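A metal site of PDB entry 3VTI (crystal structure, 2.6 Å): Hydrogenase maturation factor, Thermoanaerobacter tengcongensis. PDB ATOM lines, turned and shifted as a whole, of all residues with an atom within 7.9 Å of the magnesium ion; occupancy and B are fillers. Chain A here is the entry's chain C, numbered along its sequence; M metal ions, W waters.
Of the 20 residues printed, 3 come within 4 Å of the magnesium ion.
N of Asp 199 sits at hydrogen-bond distance from SD of Met 63.
The guanidinium group (NE) of Arg 198 lies within salt-bridge range of the side-chain carboxylate (OD2) of Asp 22, at 2.7 Å.
The side-chain hydroxyl of Thr 33 is in hydrogen-bond range of the backbone carbonyl oxygen of Asp 22, 3.2 Å away.
The magnesium ion is bound by OD1 of Asp 60 (2.0 Å), OD1 of Asp 22 (2.2 Å), OD1 of Asp 199 (2.4 Å) and water W1 (2.4 Å).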
ATOM      1  N   GLU A  21       2.667  24.160   9.076  1.00  0.00           N
ATOM      2  CA  GLU A  21       1.212  24.184   8.916  1.00  0.00           C
ATOM      3  C   GLU A  21       0.508  24.559  10.221  1.00  0.00           C
ATOM      4  O   GLU A  21       1.106  24.466  11.287  1.00  0.00           O
ATOM      5  CB  GLU A  21       0.709  22.818   8.447  1.00  0.00           C
ATOM      6  CG  GLU A  21       1.343  22.258   7.174  1.00  0.00           C
ATOM      7  CD  GLU A  21       0.799  22.882   5.899  1.00  0.00           C
ATOM      8  OE1 GLU A  21      -0.071  23.775   5.984  1.00  0.00           O
ATOM      9  OE2 GLU A  21       1.255  22.496   4.797  1.00  0.00           O
ATOM     10  N   ASP A  22      -0.752  24.974  10.102  1.00  0.00           N
ATOM     11  CA  ASP A  22      -1.633  25.206  11.256  1.00  0.00           C
ATOM     12  C   ASP A  22      -1.897  23.910  12.002  1.00  0.00           C
ATOM     13  O   ASP A  22      -2.200  23.916  13.192  1.00  0.00           O
ATOM     14  CB  ASP A  22      -2.979  25.764  10.790  1.00  0.00           C
ATOM     15  CG  ASP A  22      -2.926  27.228  10.415  1.00  0.00           C
ATOM     16  OD1 ASP A  22      -3.037  28.083  11.331  1.00  0.00           O
ATOM     17  OD2 ASP A  22      -2.774  27.530   9.204  1.00  0.00           O
ATOM     18  N   ALA A  23      -1.791  22.786  11.296  1.00  0.00           N
ATOM     19  CA  ALA A  23      -1.991  21.477  11.892  1.00  0.00           C
ATOM     20  C   ALA A  23      -1.222  20.420  11.114  1.00  0.00           C
ATOM     21  O   ALA A  23      -1.058  20.538   9.904  1.00  0.00           O
ATOM     22  CB  ALA A  23      -3.472  21.146  11.949  1.00  0.00           C
ATOM     23  N   THR A  33      -3.318  19.541  16.137  1.00  0.00           N
ATOM     24  CA  THR A  33      -2.797  20.849  16.474  1.00  0.00           C
ATOM     25  C   THR A  33      -2.652  21.015  17.981  1.00  0.00           C
ATOM     26  O   THR A  33      -3.248  20.260  18.756  1.00  0.00           O
ATOM     27  CB  THR A  33      -3.695  21.967  15.909  1.00  0.00           C
ATOM     28  OG1 THR A  33      -3.127  23.251  16.215  1.00  0.00           O
ATOM     29  CG2 THR A  33      -5.109  21.883  16.502  1.00  0.00           C
ATOM     30  N   ASP A  35      -2.076  24.488  20.945  1.00  0.00           N
ATOM     31  CA  ASP A  35      -1.790  25.880  21.244  1.00  0.00           C
ATOM     32  C   ASP A  35      -1.931  26.188  22.737  1.00  0.00           C
ATOM     33  O   ASP A  35      -2.811  25.658  23.413  1.00  0.00           O
ATOM     34  CB  ASP A  35      -2.698  26.816  20.447  1.00  0.00           C
ATOM     35  CG  ASP A  35      -2.064  28.166  20.182  1.00  0.00           C
ATOM     36  OD1 ASP A  35      -0.889  28.342  20.539  1.00  0.00           O
ATOM     37  OD2 ASP A  35      -2.730  29.051  19.610  1.00  0.00           O
ATOM     38  N   GLY A  56      -9.594  28.848  19.259  1.00  0.00           N
ATOM     39  CA  GLY A  56      -8.303  28.870  18.589  1.00  0.00           C
ATOM     40  C   GLY A  56      -7.868  27.519  18.069  1.00  0.00           C
ATOM     41  O   GLY A  56      -7.337  27.406  16.974  1.00  0.00           O
ATOM     42  N   THR A  57      -8.071  26.501  18.879  1.00  0.00           N
ATOM     43  CA  THR A  57      -7.710  25.144  18.508  1.00  0.00           C
ATOM     44  C   THR A  57      -8.731  24.502  17.576  1.00  0.00           C
ATOM     45  O   THR A  57      -8.365  23.701  16.708  1.00  0.00           O
ATOM     46  CB  THR A  57      -7.481  24.300  19.755  1.00  0.00           C
ATOM     47  OG1 THR A  57      -6.289  24.749  20.395  1.00  0.00           O
ATOM     48  CG2 THR A  57      -7.353  22.828  19.394  1.00  0.00           C
ATOM     49  N   ASN A  59     -10.296  26.249  15.410  1.00  0.00           N
ATOM     50  CA  ASN A  59      -9.935  26.911  14.181  1.00  0.00           C
ATOM     51  C   ASN A  59      -8.705  26.279  13.532  1.00  0.00           C
ATOM     52  O   ASN A  59      -8.751  25.900  12.351  1.00  0.00           O
ATOM     53  CB  ASN A  59      -9.755  28.415  14.419  1.00  0.00           C
ATOM     54  CG  ASN A  59     -11.072  29.092  14.812  1.00  0.00           C
ATOM     55  OD1 ASN A  59     -12.169  28.549  14.571  1.00  0.00           O
ATOM     56  ND2 ASN A  59     -10.981  30.279  15.419  1.00  0.00           N
ATOM     57  N   ASP A  60      -7.633  26.142  14.316  1.00  0.00           N
ATOM     58  CA  ASP A  60      -6.388  25.553  13.838  1.00  0.00           C
ATOM     59  C   ASP A  60      -6.621  24.150  13.278  1.00  0.00           C
ATOM     60  O   ASP A  60      -6.019  23.767  12.290  1.00  0.00           O
ATOM     61  CB  ASP A  60      -5.330  25.521  14.945  1.00  0.00           C
ATOM     62  CG  ASP A  60      -4.623  26.867  15.168  1.00  0.00           C
ATOM     63  OD1 ASP A  60      -4.147  27.493  14.186  1.00  0.00           O
ATOM     64  OD2 ASP A  60      -4.501  27.286  16.338  1.00  0.00           O
ATOM     65  N   ALA A  61      -7.527  23.397  13.920  1.00  0.00           N
ATOM     66  CA  ALA A  61      -7.826  22.027  13.522  1.00  0.00           C
ATOM     67  C   ALA A  61      -8.661  21.930  12.222  1.00  0.00           C
ATOM     68  O   ALA A  61      -8.809  20.840  11.658  1.00  0.00           O
ATOM     69  CB  ALA A  61      -8.508  21.283  14.652  1.00  0.00           C
ATOM     70  N   MET A  63      -8.161  24.438   9.688  1.00  0.00           N
ATOM     71  CA  MET A  63      -7.385  25.169   8.667  1.00  0.00           C
ATOM     72  C   MET A  63      -6.770  24.284   7.581  1.00  0.00           C
ATOM     73  O   MET A  63      -6.188  24.785   6.606  1.00  0.00           O
ATOM     74  CB  MET A  63      -6.288  26.001   9.312  1.00  0.00           C
ATOM     75  CG  MET A  63      -6.817  27.074  10.220  1.00  0.00           C
ATOM     76  SD  MET A  63      -7.806  28.262   9.327  1.00  0.00           S
ATOM     77  CE  MET A  63      -8.845  28.893  10.649  1.00  0.00           C
ATOM     78  N   LEU A 197      -5.875  28.105   3.952  1.00  0.00           N
ATOM     79  CA  LEU A 197      -6.710  28.602   5.027  1.00  0.00           C
ATOM     80  C   LEU A 197      -5.810  28.859   6.221  1.00  0.00           C
ATOM     81  O   LEU A 197      -5.089  27.969   6.654  1.00  0.00           O
ATOM     82  CB  LEU A 197      -7.793  27.587   5.394  1.00  0.00           C
ATOM     83  CG  LEU A 197      -8.961  27.352   4.425  1.00  0.00           C
ATOM     84  CD1 LEU A 197      -9.819  26.205   4.921  1.00  0.00           C
ATOM     85  CD2 LEU A 197      -9.815  28.595   4.251  1.00  0.00           C
ATOM     86  N   ARG A 198      -5.852  30.078   6.750  1.00  0.00           N
ATOM     87  CA  ARG A 198      -5.147  30.402   7.982  1.00  0.00           C
ATOM     88  C   ARG A 198      -5.794  31.548   8.744  1.00  0.00           C
ATOM     89  O   ARG A 198      -6.194  32.559   8.144  1.00  0.00           O
ATOM     90  CB  ARG A 198      -3.663  30.721   7.717  1.00  0.00           C
ATOM     91  CG  ARG A 198      -2.867  31.005   8.972  1.00  0.00           C
ATOM     92  CD  ARG A 198      -1.375  30.842   8.750  1.00  0.00           C
ATOM     93  NE  ARG A 198      -0.999  29.429   8.640  1.00  0.00           N
ATOM     94  CZ  ARG A 198       0.241  28.983   8.462  1.00  0.00           C
ATOM     95  NH1 ARG A 198       1.268  29.820   8.372  1.00  0.00           N
ATOM     96  NH2 ARG A 198       0.454  27.674   8.373  1.00  0.00           N
ATOM     97  N   ASP A 199      -5.912  31.383  10.052  1.00  0.00           N
ATOM     98  CA  ASP A 199      -6.396  32.448  10.925  1.00  0.00           C
ATOM     99  C   ASP A 199      -5.273  33.421  11.309  1.00  0.00           C
ATOM    100  O   ASP A 199      -4.213  32.987  11.787  1.00  0.00           O
ATOM    101  CB  ASP A 199      -7.091  31.859  12.157  1.00  0.00           C
ATOM    102  CG  ASP A 199      -6.214  30.876  12.930  1.00  0.00           C
ATOM    103  OD1 ASP A 199      -5.279  30.271  12.345  1.00  0.00           O
ATOM    104  OD2 ASP A 199      -6.499  30.716  14.145  1.00  0.00           O
ATOM    105  N   PRO A 200      -5.486  34.734  11.091  1.00  0.00           N
ATOM    106  CA  PRO A 200      -4.425  35.708  11.324  1.00  0.00           C
ATOM    107  C   PRO A 200      -4.413  36.055  12.797  1.00  0.00           C
ATOM    108  O   PRO A 200      -5.053  37.009  13.234  1.00  0.00           O
ATOM    109  CB  PRO A 200      -4.844  36.907  10.461  1.00  0.00           C
ATOM    110  CG  PRO A 200      -6.299  36.678  10.071  1.00  0.00           C
ATOM    111  CD  PRO A 200      -6.748  35.389  10.696  1.00  0.00           C
ATOM    112  N   THR A 201      -3.686  35.247  13.574  1.00  0.00           N
ATOM    113  CA  THR A 201      -3.583  35.447  15.001  1.00  0.00           C
ATOM    114  C   THR A 201      -2.281  36.234  15.267  1.00  0.00           C
ATOM    115  O   THR A 201      -2.086  37.305  14.685  1.00  0.00           O
ATOM    116  CB  THR A 201      -3.631  34.093  15.757  1.00  0.00           C
ATOM    117  OG1 THR A 201      -2.721  33.178  15.153  1.00  0.00           O
ATOM    118  CG2 THR A 201      -5.032  33.464  15.695  1.00  0.00           C
ATOM    119  N   ARG A 202      -1.409  35.718  16.109  1.00  0.00           N
ATOM    120  CA  ARG A 202      -0.147  36.406  16.414  1.00  0.00           C
ATOM    121  C   ARG A 202       0.571  36.978  15.193  1.00  0.00           C
ATOM    122  O   ARG A 202       1.178  36.231  14.416  1.00  0.00           O
ATOM    123  CB  ARG A 202       0.803  35.483  17.186  1.00  0.00           C
ATOM    124  CG  ARG A 202       2.155  36.137  17.541  1.00  0.00           C
ATOM    125  CD  ARG A 202       2.206  36.610  19.012  1.00  0.00           C
ATOM    126  NE  ARG A 202       3.451  37.337  19.344  1.00  0.00           N
ATOM    127  CZ  ARG A 202       4.679  36.808  19.332  1.00  0.00           C
ATOM    128  NH1 ARG A 202       4.892  35.539  18.979  1.00  0.00           N
ATOM    129  NH2 ARG A 202       5.731  37.573  19.651  1.00  0.00           N
ATOM    130  N   VAL A 208       0.443  36.245   8.185  1.00  0.00           N
ATOM    131  CA  VAL A 208      -0.139  35.196   7.357  1.00  0.00           C
ATOM    132  C   VAL A 208       0.310  35.322   5.885  1.00  0.00           C
ATOM    133  O   VAL A 208       0.767  34.348   5.290  1.00  0.00           O
ATOM    134  CB  VAL A 208      -1.691  35.212   7.456  1.00  0.00           C
ATOM    135  CG1 VAL A 208      -2.333  34.369   6.325  1.00  0.00           C
ATOM    136  CG2 VAL A 208      -2.158  34.728   8.825  1.00  0.00           C
ATOM    137  N   GLU A 211       3.742  34.304   5.433  1.00  0.00           N
ATOM    138  CA  GLU A 211       3.862  32.856   5.605  1.00  0.00           C
ATOM    139  C   GLU A 211       3.407  32.143   4.337  1.00  0.00           C
ATOM    140  O   GLU A 211       4.008  31.138   3.943  1.00  0.00           O
ATOM    141  CB  GLU A 211       3.058  32.380   6.811  1.00  0.00           C
ATOM    142  CG  GLU A 211       3.746  32.667   8.148  1.00  0.00           C
ATOM    143  CD  GLU A 211       2.790  32.727   9.337  1.00  0.00           C
ATOM    144  OE1 GLU A 211       1.553  32.736   9.140  1.00  0.00           O
ATOM    145  OE2 GLU A 211       3.286  32.762  10.483  1.00  0.00           O
ATOM    146  N   GLU A 250      -9.240  36.638  16.145  1.00  0.00           N
ATOM    147  CA  GLU A 250      -9.573  35.328  16.729  1.00  0.00           C
ATOM    148  C   GLU A 250     -10.903  34.780  16.224  1.00  0.00           C
ATOM    149  O   GLU A 250     -11.356  33.726  16.676  1.00  0.00           O
ATOM    150  CB  GLU A 250      -9.565  35.377  18.267  1.00  0.00           C
ATOM    151  CG  GLU A 250      -8.180  35.557  18.903  1.00  0.00           C
ATOM    152  CD  GLU A 250      -7.234  34.393  18.641  1.00  0.00           C
ATOM    153  OE1 GLU A 250      -7.699  33.290  18.290  1.00  0.00           O
ATOM    154  OE2 GLU A 250      -6.009  34.586  18.812  1.00  0.00           O
HETATM  155 MG    MG M   1      -3.384  29.136  13.244  1.00  0.00          MG
HETATM  156  O   HOH W   1      -1.202  28.175  13.435  1.00  0.00           O
